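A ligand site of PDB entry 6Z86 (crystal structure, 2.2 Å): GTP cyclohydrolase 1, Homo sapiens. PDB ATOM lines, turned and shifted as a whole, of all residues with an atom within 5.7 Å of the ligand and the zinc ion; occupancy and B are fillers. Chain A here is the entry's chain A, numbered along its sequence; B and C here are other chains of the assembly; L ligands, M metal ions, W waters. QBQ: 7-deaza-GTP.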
ATOM      1  N   LEU A  91     -24.615  -6.008  10.341  1.00  0.00           N
ATOM      2  CA  LEU A  91     -25.383  -5.406   9.251  1.00  0.00           C
ATOM      3  C   LEU A  91     -24.938  -3.988   8.865  1.00  0.00           C
ATOM      4  O   LEU A  91     -25.000  -3.638   7.691  1.00  0.00           O
ATOM      5  CB  LEU A  91     -26.882  -5.399   9.541  1.00  0.00           C
ATOM      6  CG  LEU A  91     -27.528  -6.744   9.817  1.00  0.00           C
ATOM      7  CD1 LEU A  91     -28.973  -6.564  10.226  1.00  0.00           C
ATOM      8  CD2 LEU A  91     -27.413  -7.667   8.630  1.00  0.00           C
ATOM      9  N   ASN A  92     -24.538  -3.162   9.858  1.00  0.00           N
ATOM     10  CA  ASN A  92     -24.048  -1.788   9.649  1.00  0.00           C
ATOM     11  C   ASN A  92     -25.019  -0.933   8.836  1.00  0.00           C
ATOM     12  O   ASN A  92     -24.594  -0.116   8.038  1.00  0.00           O
ATOM     13  CB  ASN A  92     -22.653  -1.810   8.999  1.00  0.00           C
ATOM     14  CG  ASN A  92     -21.881  -0.529   9.114  1.00  0.00           C
ATOM     15  OD1 ASN A  92     -21.963   0.184  10.116  1.00  0.00           O
ATOM     16  ND2 ASN A  92     -21.117  -0.196   8.092  1.00  0.00           N
ATOM     17  N   ALA A  94     -26.765  -1.702   6.302  1.00  0.00           N
ATOM     18  CA  ALA A  94     -26.658  -1.936   4.868  1.00  0.00           C
ATOM     19  C   ALA A  94     -27.925  -2.635   4.399  1.00  0.00           C
ATOM     20  O   ALA A  94     -27.870  -3.630   3.709  1.00  0.00           O
ATOM     21  CB  ALA A  94     -25.424  -2.749   4.539  1.00  0.00           C
ATOM     22  N   PHE A  96     -30.833  -1.580   2.217  1.00  0.00           N
ATOM     23  CA  PHE A  96     -31.247  -0.570   1.243  1.00  0.00           C
ATOM     24  C   PHE A  96     -32.729  -0.674   0.919  1.00  0.00           C
ATOM     25  O   PHE A  96     -33.380  -1.677   1.229  1.00  0.00           O
ATOM     26  CB  PHE A  96     -30.393  -0.657  -0.052  1.00  0.00           C
ATOM     27  CG  PHE A  96     -28.919  -0.820   0.237  1.00  0.00           C
ATOM     28  CD1 PHE A  96     -28.216   0.168   0.892  1.00  0.00           C
ATOM     29  CD2 PHE A  96     -28.272  -2.018  -0.024  1.00  0.00           C
ATOM     30  CE1 PHE A  96     -26.883  -0.017   1.243  1.00  0.00           C
ATOM     31  CE2 PHE A  96     -26.937  -2.195   0.304  1.00  0.00           C
ATOM     32  CZ  PHE A  96     -26.254  -1.191   0.940  1.00  0.00           C
ATOM     33  N   TYR A 130     -32.767 -15.387  -1.268  1.00  0.00           N
ATOM     34  CA  TYR A 130     -33.878 -14.741  -0.574  1.00  0.00           C
ATOM     35  C   TYR A 130     -34.756 -13.948  -1.527  1.00  0.00           C
ATOM     36  O   TYR A 130     -34.326 -13.560  -2.611  1.00  0.00           O
ATOM     37  CB  TYR A 130     -33.425 -13.910   0.645  1.00  0.00           C
ATOM     38  CG  TYR A 130     -32.860 -12.544   0.315  1.00  0.00           C
ATOM     39  CD1 TYR A 130     -31.550 -12.384  -0.093  1.00  0.00           C
ATOM     40  CD2 TYR A 130     -33.644 -11.400   0.479  1.00  0.00           C
ATOM     41  CE1 TYR A 130     -31.038 -11.129  -0.409  1.00  0.00           C
ATOM     42  CE2 TYR A 130     -33.133 -10.142   0.177  1.00  0.00           C
ATOM     43  CZ  TYR A 130     -31.833 -10.005  -0.271  1.00  0.00           C
ATOM     44  OH  TYR A 130     -31.301  -8.775  -0.560  1.00  0.00           O
ATOM     45  N   VAL A 136     -33.639  -4.628   0.021  1.00  0.00           N
ATOM     46  CA  VAL A 136     -32.569  -5.580  -0.178  1.00  0.00           C
ATOM     47  C   VAL A 136     -31.455  -5.400   0.833  1.00  0.00           C
ATOM     48  O   VAL A 136     -31.221  -4.298   1.295  1.00  0.00           O
ATOM     49  CB  VAL A 136     -32.003  -5.512  -1.598  1.00  0.00           C
ATOM     50  CG1 VAL A 136     -33.024  -5.999  -2.620  1.00  0.00           C
ATOM     51  CG2 VAL A 136     -31.528  -4.099  -1.930  1.00  0.00           C
ATOM     52  N   LEU A 137     -30.743  -6.468   1.132  1.00  0.00           N
ATOM     53  CA  LEU A 137     -29.608  -6.416   2.045  1.00  0.00           C
ATOM     54  C   LEU A 137     -28.330  -6.234   1.212  1.00  0.00           C
ATOM     55  O   LEU A 137     -28.215  -6.741   0.085  1.00  0.00           O
ATOM     56  CB  LEU A 137     -29.513  -7.757   2.800  1.00  0.00           C
ATOM     57  CG  LEU A 137     -28.589  -7.829   4.023  1.00  0.00           C
ATOM     58  CD1 LEU A 137     -28.905  -6.735   5.039  1.00  0.00           C
ATOM     59  CD2 LEU A 137     -28.709  -9.170   4.722  1.00  0.00           C
ATOM     60  N   GLY A 138     -27.332  -5.612   1.835  1.00  0.00           N
ATOM     61  CA  GLY A 138     -25.989  -5.504   1.302  1.00  0.00           C
ATOM     62  C   GLY A 138     -25.450  -6.905   1.101  1.00  0.00           C
ATOM     63  O   GLY A 138     -25.736  -7.780   1.928  1.00  0.00           O
ATOM     64  N   LEU A 139     -24.857  -7.180  -0.050  1.00  0.00           N
ATOM     65  CA  LEU A 139     -24.435  -8.540  -0.399  1.00  0.00           C
ATOM     66  C   LEU A 139     -23.469  -9.131   0.578  1.00  0.00           C
ATOM     67  O   LEU A 139     -23.584 -10.304   0.911  1.00  0.00           O
ATOM     68  CB  LEU A 139     -23.811  -8.568  -1.804  1.00  0.00           C
ATOM     69  CG  LEU A 139     -24.662  -8.164  -2.969  1.00  0.00           C
ATOM     70  CD1 LEU A 139     -23.817  -8.165  -4.250  1.00  0.00           C
ATOM     71  CD2 LEU A 139     -25.890  -9.043  -3.101  1.00  0.00           C
ATOM     72  N   SER A 140     -22.453  -8.352   0.981  1.00  0.00           N
ATOM     73  CA  SER A 140     -21.429  -8.882   1.874  1.00  0.00           C
ATOM     74  C   SER A 140     -21.979  -9.264   3.226  1.00  0.00           C
ATOM     75  O   SER A 140     -21.382 -10.089   3.905  1.00  0.00           O
ATOM     76  CB  SER A 140     -20.283  -7.884   2.014  1.00  0.00           C
ATOM     77  OG  SER A 140     -20.735  -6.770   2.776  1.00  0.00           O
ATOM     78  N   LYS A 141     -23.086  -8.633   3.656  1.00  0.00           N
ATOM     79  CA  LYS A 141     -23.701  -8.904   4.955  1.00  0.00           C
ATOM     80  C   LYS A 141     -24.218 -10.357   5.052  1.00  0.00           C
ATOM     81  O   LYS A 141     -24.186 -10.933   6.147  1.00  0.00           O
ATOM     82  CB  LYS A 141     -24.780  -7.856   5.280  1.00  0.00           C
ATOM     83  CG  LYS A 141     -24.305  -6.407   5.072  1.00  0.00           C
ATOM     84  CD  LYS A 141     -23.051  -6.010   5.886  1.00  0.00           C
ATOM     85  CE  LYS A 141     -22.533  -4.638   5.500  1.00  0.00           C
ATOM     86  NZ  LYS A 141     -21.296  -4.260   6.244  1.00  0.00           N
ATOM     87  N   ARG A 144     -21.194 -12.147   6.009  1.00  0.00           N
ATOM     88  CA  ARG A 144     -20.882 -11.779   7.380  1.00  0.00           C
ATOM     89  C   ARG A 144     -21.808 -12.482   8.407  1.00  0.00           C
ATOM     90  O   ARG A 144     -21.378 -12.758   9.539  1.00  0.00           O
ATOM     91  CB  ARG A 144     -20.931 -10.259   7.557  1.00  0.00           C
ATOM     92  CG  ARG A 144     -19.834  -9.538   6.803  1.00  0.00           C
ATOM     93  CD  ARG A 144     -19.790  -8.053   7.131  1.00  0.00           C
ATOM     94  NE  ARG A 144     -18.701  -7.344   6.451  1.00  0.00           N
ATOM     95  CZ  ARG A 144     -17.423  -7.355   6.840  1.00  0.00           C
ATOM     96  NH1 ARG A 144     -17.050  -8.094   7.879  1.00  0.00           N
ATOM     97  NH2 ARG A 144     -16.511  -6.658   6.174  1.00  0.00           N
ATOM     98  N   CYS B 115     -19.099  -1.155  -8.771  1.00  0.00           N
ATOM     99  CA  CYS B 115     -19.845  -1.096  -7.526  1.00  0.00           C
ATOM    100  C   CYS B 115     -19.997   0.376  -7.099  1.00  0.00           C
ATOM    101  O   CYS B 115     -18.992   1.074  -6.964  1.00  0.00           O
ATOM    102  CB  CYS B 115     -19.142  -1.917  -6.456  1.00  0.00           C
ATOM    103  SG  CYS B 115     -19.683  -1.581  -4.763  1.00  0.00           S
ATOM    104  N   GLU B 116     -21.237   0.846  -6.921  1.00  0.00           N
ATOM    105  CA  GLU B 116     -21.448   2.246  -6.523  1.00  0.00           C
ATOM    106  C   GLU B 116     -21.116   2.506  -5.045  1.00  0.00           C
ATOM    107  O   GLU B 116     -21.035   3.659  -4.657  1.00  0.00           O
ATOM    108  CB  GLU B 116     -22.871   2.700  -6.842  1.00  0.00           C
ATOM    109  CG  GLU B 116     -23.931   2.093  -5.932  1.00  0.00           C
ATOM    110  CD  GLU B 116     -25.352   2.489  -6.299  1.00  0.00           C
ATOM    111  OE1 GLU B 116     -26.255   2.290  -5.450  1.00  0.00           O
ATOM    112  OE2 GLU B 116     -25.569   2.981  -7.426  1.00  0.00           O
ATOM    113  N   HIS B 117     -20.939   1.452  -4.230  1.00  0.00           N
ATOM    114  CA  HIS B 117     -20.621   1.625  -2.824  1.00  0.00           C
ATOM    115  C   HIS B 117     -19.126   1.791  -2.546  1.00  0.00           C
ATOM    116  O   HIS B 117     -18.766   2.538  -1.645  1.00  0.00           O
ATOM    117  CB  HIS B 117     -21.227   0.494  -1.991  1.00  0.00           C
ATOM    118  CG  HIS B 117     -22.728   0.498  -2.018  1.00  0.00           C
ATOM    119  ND1 HIS B 117     -23.467   1.274  -1.153  1.00  0.00           N
ATOM    120  CD2 HIS B 117     -23.571  -0.139  -2.861  1.00  0.00           C
ATOM    121  CE1 HIS B 117     -24.738   1.079  -1.478  1.00  0.00           C
ATOM    122  NE2 HIS B 117     -24.847   0.223  -2.495  1.00  0.00           N
ATOM    123  N   HIS B 118     -18.257   1.125  -3.323  1.00  0.00           N
ATOM    124  CA  HIS B 118     -16.811   1.209  -3.107  1.00  0.00           C
ATOM    125  C   HIS B 118     -16.017   1.692  -4.310  1.00  0.00           C
ATOM    126  O   HIS B 118     -14.802   1.889  -4.172  1.00  0.00           O
ATOM    127  CB  HIS B 118     -16.242  -0.157  -2.678  1.00  0.00           C
ATOM    128  CG  HIS B 118     -16.809  -0.687  -1.395  1.00  0.00           C
ATOM    129  ND1 HIS B 118     -17.838  -1.610  -1.393  1.00  0.00           N
ATOM    130  CD2 HIS B 118     -16.462  -0.406  -0.113  1.00  0.00           C
ATOM    131  CE1 HIS B 118     -18.100  -1.857  -0.122  1.00  0.00           C
ATOM    132  NE2 HIS B 118     -17.297  -1.153   0.684  1.00  0.00           N
ATOM    133  N   LEU B 119     -16.654   1.795  -5.483  1.00  0.00           N
ATOM    134  CA  LEU B 119     -16.014   2.180  -6.741  1.00  0.00           C
ATOM    135  C   LEU B 119     -14.925   1.179  -7.153  1.00  0.00           C
ATOM    136  O   LEU B 119     -13.841   1.542  -7.595  1.00  0.00           O
ATOM    137  CB  LEU B 119     -15.510   3.641  -6.719  1.00  0.00           C
ATOM    138  CG  LEU B 119     -16.554   4.700  -6.385  1.00  0.00           C
ATOM    139  CD1 LEU B 119     -15.944   6.079  -6.468  1.00  0.00           C
ATOM    140  CD2 LEU B 119     -17.737   4.658  -7.339  1.00  0.00           C
ATOM    141  N   VAL B 120     -15.236  -0.099  -7.001  1.00  0.00           N
ATOM    142  CA  VAL B 120     -14.414  -1.240  -7.356  1.00  0.00           C
ATOM    143  C   VAL B 120     -15.253  -2.099  -8.334  1.00  0.00           C
ATOM    144  O   VAL B 120     -16.478  -2.158  -8.195  1.00  0.00           O
ATOM    145  CB  VAL B 120     -14.023  -2.008  -6.058  1.00  0.00           C
ATOM    146  CG1 VAL B 120     -13.326  -3.311  -6.340  1.00  0.00           C
ATOM    147  CG2 VAL B 120     -13.160  -1.161  -5.148  1.00  0.00           C
ATOM    148  N   PHE B 122     -17.326  -5.008 -10.470  1.00  0.00           N
ATOM    149  CA  PHE B 122     -18.044  -6.254 -10.298  1.00  0.00           C
ATOM    150  C   PHE B 122     -18.270  -6.773 -11.729  1.00  0.00           C
ATOM    151  O   PHE B 122     -18.698  -6.025 -12.610  1.00  0.00           O
ATOM    152  CB  PHE B 122     -19.298  -6.182  -9.420  1.00  0.00           C
ATOM    153  CG  PHE B 122     -20.545  -5.516  -9.946  1.00  0.00           C
ATOM    154  CD1 PHE B 122     -21.502  -6.253 -10.624  1.00  0.00           C
ATOM    155  CD2 PHE B 122     -20.838  -4.199  -9.628  1.00  0.00           C
ATOM    156  CE1 PHE B 122     -22.694  -5.659 -11.039  1.00  0.00           C
ATOM    157  CE2 PHE B 122     -22.017  -3.603 -10.049  1.00  0.00           C
ATOM    158  CZ  PHE B 122     -22.948  -4.337 -10.754  1.00  0.00           C
ATOM    159  N   GLN B 154     -23.177   1.063 -10.310  1.00  0.00           N
ATOM    160  CA  GLN B 154     -24.325   0.200 -10.142  1.00  0.00           C
ATOM    161  C   GLN B 154     -24.440  -0.587  -8.845  1.00  0.00           C
ATOM    162  O   GLN B 154     -23.534  -0.656  -8.013  1.00  0.00           O
ATOM    163  CB  GLN B 154     -24.324  -0.799 -11.327  1.00  0.00           C
ATOM    164  CG  GLN B 154     -24.901  -0.266 -12.617  1.00  0.00           C
ATOM    165  CD  GLN B 154     -26.390  -0.098 -12.577  1.00  0.00           C
ATOM    166  OE1 GLN B 154     -27.052  -0.163 -11.527  1.00  0.00           O
ATOM    167  NE2 GLN B 154     -26.977   0.134 -13.731  1.00  0.00           N
ATOM    168  N   VAL B 155     -25.602  -1.225  -8.717  1.00  0.00           N
ATOM    169  CA  VAL B 155     -25.992  -2.237  -7.782  1.00  0.00           C
ATOM    170  C   VAL B 155     -26.572  -3.340  -8.737  1.00  0.00           C
ATOM    171  O   VAL B 155     -27.315  -3.027  -9.682  1.00  0.00           O
ATOM    172  CB  VAL B 155     -26.978  -1.645  -6.744  1.00  0.00           C
ATOM    173  CG1 VAL B 155     -28.187  -2.530  -6.499  1.00  0.00           C
ATOM    174  CG2 VAL B 155     -26.248  -1.323  -5.441  1.00  0.00           C
ATOM    175  N   GLN B 156     -26.090  -4.598  -8.593  1.00  0.00           N
ATOM    176  CA  GLN B 156     -26.464  -5.704  -9.464  1.00  0.00           C
ATOM    177  C   GLN B 156     -27.963  -5.896  -9.652  1.00  0.00           C
ATOM    178  O   GLN B 156     -28.404  -6.201 -10.765  1.00  0.00           O
ATOM    179  CB  GLN B 156     -25.808  -7.007  -9.000  1.00  0.00           C
ATOM    180  CG  GLN B 156     -25.904  -8.118 -10.024  1.00  0.00           C
ATOM    181  CD  GLN B 156     -25.158  -9.359  -9.627  1.00  0.00           C
ATOM    182  OE1 GLN B 156     -24.110  -9.289  -8.986  1.00  0.00           O
ATOM    183  NE2 GLN B 156     -25.669 -10.515 -10.019  1.00  0.00           N
ATOM    184  N   GLU B 157     -28.745  -5.734  -8.579  1.00  0.00           N
ATOM    185  CA  GLU B 157     -30.192  -5.865  -8.628  1.00  0.00           C
ATOM    186  C   GLU B 157     -30.819  -4.821  -9.549  1.00  0.00           C
ATOM    187  O   GLU B 157     -31.731  -5.140 -10.316  1.00  0.00           O
ATOM    188  CB  GLU B 157     -30.784  -5.747  -7.220  1.00  0.00           C
ATOM    189  CG  GLU B 157     -30.364  -6.896  -6.315  1.00  0.00           C
ATOM    190  CD  GLU B 157     -29.188  -6.622  -5.416  1.00  0.00           C
ATOM    191  OE1 GLU B 157     -29.217  -7.093  -4.258  1.00  0.00           O
ATOM    192  OE2 GLU B 157     -28.237  -5.933  -5.839  1.00  0.00           O
ATOM    193  N   HIS B 184     -18.023  -9.805  -7.207  1.00  0.00           N
ATOM    194  CA  HIS B 184     -17.826  -8.454  -6.727  1.00  0.00           C
ATOM    195  C   HIS B 184     -16.447  -8.434  -6.117  1.00  0.00           C
ATOM    196  O   HIS B 184     -16.218  -9.142  -5.140  1.00  0.00           O
ATOM    197  CB  HIS B 184     -18.882  -8.101  -5.676  1.00  0.00           C
ATOM    198  CG  HIS B 184     -20.247  -7.833  -6.246  1.00  0.00           C
ATOM    199  ND1 HIS B 184     -20.827  -6.590  -6.166  1.00  0.00           N
ATOM    200  CD2 HIS B 184     -21.077  -8.669  -6.903  1.00  0.00           C
ATOM    201  CE1 HIS B 184     -22.003  -6.707  -6.762  1.00  0.00           C
ATOM    202  NE2 HIS B 184     -22.189  -7.926  -7.235  1.00  0.00           N
ATOM    203  N   CYS B 186     -15.170  -6.192  -4.325  1.00  0.00           N
ATOM    204  CA  CYS B 186     -15.358  -5.693  -2.950  1.00  0.00           C
ATOM    205  C   CYS B 186     -15.503  -6.819  -1.959  1.00  0.00           C
ATOM    206  O   CYS B 186     -15.347  -6.574  -0.761  1.00  0.00           O
ATOM    207  CB  CYS B 186     -16.575  -4.789  -2.866  1.00  0.00           C
ATOM    208  SG  CYS B 186     -16.633  -3.526  -4.138  1.00  0.00           S
ATOM    209  N   MET B 187     -15.933  -7.996  -2.419  1.00  0.00           N
ATOM    210  CA  MET B 187     -16.094  -9.133  -1.557  1.00  0.00           C
ATOM    211  C   MET B 187     -14.937 -10.121  -1.662  1.00  0.00           C
ATOM    212  O   MET B 187     -14.852 -10.982  -0.816  1.00  0.00           O
ATOM    213  CB  MET B 187     -17.432  -9.837  -1.851  1.00  0.00           C
ATOM    214  CG  MET B 187     -18.648  -8.928  -1.717  1.00  0.00           C
ATOM    215  SD  MET B 187     -20.156  -9.896  -1.486  1.00  0.00           S
ATOM    216  CE  MET B 187     -20.489 -10.431  -3.177  1.00  0.00           C
ATOM    217  N   ARG B 190     -11.137  -7.555  -0.493  1.00  0.00           N
ATOM    218  CA  ARG B 190     -11.332  -6.664   0.620  1.00  0.00           C
ATOM    219  C   ARG B 190     -12.584  -7.141   1.411  1.00  0.00           C
ATOM    220  O   ARG B 190     -13.263  -8.076   0.994  1.00  0.00           O
ATOM    221  CB  ARG B 190     -11.623  -5.299  -0.036  1.00  0.00           C
ATOM    222  CG  ARG B 190     -11.516  -4.085   0.812  1.00  0.00           C
ATOM    223  CD  ARG B 190     -12.500  -3.022   0.330  1.00  0.00           C
ATOM    224  NE  ARG B 190     -13.867  -3.550   0.291  1.00  0.00           N
ATOM    225  CZ  ARG B 190     -14.715  -3.571   1.309  1.00  0.00           C
ATOM    226  NH1 ARG B 190     -15.925  -4.094   1.154  1.00  0.00           N
ATOM    227  NH2 ARG B 190     -14.366  -3.071   2.489  1.00  0.00           N
ATOM    228  N   GLY B 191     -12.867  -6.475   2.539  1.00  0.00           N
ATOM    229  CA  GLY B 191     -14.028  -6.738   3.382  1.00  0.00           C
ATOM    230  C   GLY B 191     -14.115  -8.148   3.901  1.00  0.00           C
ATOM    231  O   GLY B 191     -13.255  -8.608   4.673  1.00  0.00           O
ATOM    232  N   VAL B 192     -15.136  -8.861   3.465  1.00  0.00           N
ATOM    233  CA  VAL B 192     -15.401 -10.215   3.879  1.00  0.00           C
ATOM    234  C   VAL B 192     -14.381 -11.216   3.288  1.00  0.00           C
ATOM    235  O   VAL B 192     -14.146 -12.272   3.886  1.00  0.00           O
ATOM    236  CB  VAL B 192     -16.857 -10.547   3.539  1.00  0.00           C
ATOM    237  CG1 VAL B 192     -17.007 -10.913   2.059  1.00  0.00           C
ATOM    238  CG2 VAL B 192     -17.410 -11.610   4.452  1.00  0.00           C
ATOM    239  N   LYS C  67     -22.627   7.295   1.325  1.00  0.00           N
ATOM    240  CA  LYS C  67     -21.439   6.866   2.086  1.00  0.00           C
ATOM    241  C   LYS C  67     -20.244   6.492   1.189  1.00  0.00           C
ATOM    242  O   LYS C  67     -19.179   6.193   1.729  1.00  0.00           O
ATOM    243  CB  LYS C  67     -21.763   5.714   3.051  1.00  0.00           C
ATOM    244  CG  LYS C  67     -22.853   6.013   4.064  1.00  0.00           C
ATOM    245  CD  LYS C  67     -22.337   6.046   5.519  1.00  0.00           C
ATOM    246  CE  LYS C  67     -21.811   7.414   5.970  1.00  0.00           C
ATOM    247  NZ  LYS C  67     -20.859   7.301   7.124  1.00  0.00           N
ATOM    248  N   ARG C  71     -16.463   4.925   1.941  1.00  0.00           N
ATOM    249  CA  ARG C  71     -16.232   3.507   1.671  1.00  0.00           C
ATOM    250  C   ARG C  71     -15.161   3.320   0.601  1.00  0.00           C
ATOM    251  O   ARG C  71     -14.381   2.383   0.690  1.00  0.00           O
ATOM    252  CB  ARG C  71     -17.524   2.769   1.264  1.00  0.00           C
ATOM    253  CG  ARG C  71     -18.714   2.874   2.214  1.00  0.00           C
ATOM    254  CD  ARG C  71     -18.491   2.258   3.572  1.00  0.00           C
ATOM    255  NE  ARG C  71     -18.461   3.272   4.634  1.00  0.00           N
ATOM    256  CZ  ARG C  71     -19.392   3.412   5.567  1.00  0.00           C
ATOM    257  NH1 ARG C  71     -19.285   4.376   6.480  1.00  0.00           N
ATOM    258  NH2 ARG C  71     -20.442   2.612   5.604  1.00  0.00           N
HETATM  259  O3  QBQ L   1     -21.856   0.561   4.270  1.00  0.00           O
HETATM  260  C4  QBQ L   1     -22.424  -3.341  -2.698  1.00  0.00           C
HETATM  261  C5  QBQ L   1     -23.251  -3.950  -0.375  1.00  0.00           C
HETATM  262  O4  QBQ L   1     -19.875  -0.924   3.845  1.00  0.00           O
HETATM  263  C6  QBQ L   1     -22.982  -2.885   1.616  1.00  0.00           C
HETATM  264  N1  QBQ L   1     -25.631  -4.652  -2.008  1.00  0.00           N
HETATM  265  C7  QBQ L   1     -22.353  -1.610   2.093  1.00  0.00           C
HETATM  266  C8  QBQ L   1     -22.065  -4.109   1.601  1.00  0.00           C
HETATM  267  N2  QBQ L   1     -23.404  -3.771  -1.817  1.00  0.00           N
HETATM  268  C9  QBQ L   1     -21.877  -4.376   0.093  1.00  0.00           C
HETATM  269  O5  QBQ L   1     -17.386  -1.182   3.425  1.00  0.00           O
HETATM  270  C10 QBQ L   1     -25.050  -4.729  -4.835  1.00  0.00           C
HETATM  271  O6  QBQ L   1     -18.429  -1.732   5.775  1.00  0.00           O
HETATM  272  N3  QBQ L   1     -26.253  -5.111  -4.257  1.00  0.00           N
HETATM  273  O7  QBQ L   1     -18.957  -3.168   3.773  1.00  0.00           O
HETATM  274  O8  QBQ L   1     -18.062  -4.952   2.251  1.00  0.00           O
HETATM  275  N   QBQ L   1     -27.694  -5.553  -2.510  1.00  0.00           N
HETATM  276  C   QBQ L   1     -26.510  -5.075  -2.919  1.00  0.00           C
HETATM  277  O   QBQ L   1     -23.483  -2.727   0.274  1.00  0.00           O
HETATM  278  C1  QBQ L   1     -24.460  -4.253  -2.548  1.00  0.00           C
HETATM  279  C2  QBQ L   1     -24.101  -4.218  -3.896  1.00  0.00           C
HETATM  280  C3  QBQ L   1     -22.806  -3.631  -3.975  1.00  0.00           C
HETATM  281  O1  QBQ L   1     -22.266  -1.751   3.515  1.00  0.00           O
HETATM  282  O10 QBQ L   1     -19.182  -5.531   4.441  1.00  0.00           O
HETATM  283  O11 QBQ L   1     -22.786  -5.168   2.224  1.00  0.00           O
HETATM  284  O12 QBQ L   1     -21.479  -5.693  -0.286  1.00  0.00           O
HETATM  285  O13 QBQ L   1     -24.833  -4.939  -6.033  1.00  0.00           O
HETATM  286  O2  QBQ L   1     -21.326  -1.464   5.817  1.00  0.00           O
HETATM  287  O9  QBQ L   1     -16.930  -4.414   4.485  1.00  0.00           O
HETATM  288  P   QBQ L   1     -21.354  -0.853   4.428  1.00  0.00           P
HETATM  289  P1  QBQ L   1     -18.573  -1.718   4.290  1.00  0.00           P
HETATM  290  P2  QBQ L   1     -18.240  -4.582   3.706  1.00  0.00           P
HETATM  291 ZN    ZN M   1     -18.518  -2.839  -3.179  1.00  0.00          ZN
HETATM  292  O   HOH W   1     -15.842  -2.861   6.752  1.00  0.00           O
HETATM  293  O   HOH W   2     -18.525  -3.026   7.981  1.00  0.00           O
HETATM  294  O   HOH W   3     -19.753  -5.258  -2.949  1.00  0.00           O
HETATM  295  O   HOH W   4     -16.918  -7.482   1.607  1.00  0.00           O
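Three residues have an atom within 4 Å of the zinc ion: Cys 115 of chain B, His 118 of chain B and Cys 186 of chain B. The nearest printed residue that does not touch the zinc ion is His 117 of chain B (4.5 Å).
An oxygen (O2) of the ligand lies within salt-bridge range of the side-chain amino group (NZ) of Lys 141, 2.8 Å away. An oxygen (O12) of the ligand sits at hydrogen-bond distance from the backbone NH (N) of Ser 140, at 3.1 Å. O8 of the ligand is in salt-bridge range of NH1 of Arg 190 of chain B, 2.6 Å away. The side-chain carboxylate (OE2) of Glu 157 of chain B sits at hydrogen-bond distance from a nitrogen (N3) of the ligand (2.7 Å). N of Leu 139 is in hydrogen-bond range of N1 of the ligand (3.3 Å). A ring nitrogen (NE2) of His 118 of chain B is in hydrogen-bond range of an oxygen (O5) of the ligand. The guanidinium group (NH2) of Arg 71 of chain C is in salt-bridge range of an oxygen (O3) of the ligand, 2.8 Å away. The backbone NH of Gln 156 of chain B lies within hydrogen-bond range of an oxygen (O13) of the ligand (2.9 Å). The side-chain hydroxyl (OG) of Ser 140 lies within hydrogen-bond range of an oxygen (O10) of the ligand (2.6 Å). The side-chain amide nitrogen of Asn 92 is in hydrogen-bond range of an oxygen (O2) of the ligand (2.6 Å). The backbone carbonyl oxygen (O) of Leu 137 lies within hydrogen-bond range of a nitrogen (N) of the ligand, at 2.9 Å. The guanidinium group (NE) of Arg 144 is in salt-bridge range of an oxygen (O10) of the ligand, at 2.7 Å.
Water W2 bridges an oxygen (O6) of the ligand (2.6 Å) and the side-chain amino group of Lys 141 (3.5 Å). Water W4 lies within hydrogen-bond range of O8 of the ligand (2.9 Å), N of Val 192 of chain B (2.9 Å) and O of Cys 186 of chain B (3.0 Å).
Residues that only touch the ligand: Ala 94 (3.5 Å), Phe 96 (3.2 Å), Gly 138 (3.3 Å), His 117 of chain B (3.4 Å), Val 155 of chain B (3.4 Å), His 184 of chain B (3.4 Å) and Gly 191 of chain B (3.9 Å). Hydrophobic or aromatic side chains that line the ligand: Ala 94, Phe 96, Leu 139, His 117 of chain B, His 118 of chain B, Val 155 of chain B and His 184 of chain B. 19 residues have an atom within 4 Å of the ligand: Asn 92, Ala 94, Phe 96, Leu 137, Gly 138, Leu 139, Ser 140, Lys 141, Arg 144, Cys 115 of chain B, His 117 of chain B, His 118 of chain B, Val 155 of chain B, Gln 156 of chain B, Glu 157 of chain B, His 184 of chain B, Arg 190 of chain B, Gly 191 of chain B and Arg 71 of chain C.
The side-chain amide oxygen (OE1) of Gln 156 of chain B sits at hydrogen-bond distance from a ring nitrogen (NE2) of His 184 of chain B. The backbone carbonyl oxygen (O) of Cys 186 of chain B sits at hydrogen-bond distance from the guanidinium group (NH1) of Arg 190 of chain B (3.2 Å). The backbone NH (N) of Gly 138 sits at hydrogen-bond distance from the backbone carbonyl oxygen (O) of Ala 94 (2.8 Å). N of Ser 140 is in hydrogen-bond range of SD of Met 187 of chain B (3.7 Å). The side-chain hydroxyl (OH) of Tyr 130 sits at hydrogen-bond distance from the backbone NH (N) of Leu 137, 2.9 Å away. The backbone NH (N) of His 117 of chain B lies close to the side-chain sulfur (SG) of Cys 115 of chain B (3.3 Å). NE2 of His 118 of chain B sits at hydrogen-bond distance from NH1 of Arg 190 of chain B (3.3 Å). The backbone NH (N) of Phe 96 sits at hydrogen-bond distance from the backbone carbonyl oxygen (O) of Val 136.
The side-chain sulfur (SG) of Cys 186 of chain B is bound to the zinc ion. A ring nitrogen (ND1) of His 118 of chain B is bound to the zinc ion (2.3 Å). SG of Cys 115 of chain B is bound to the zinc ion (2.3 Å). Slightly farther from the zinc ion lies water W3 (2.7 Å).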
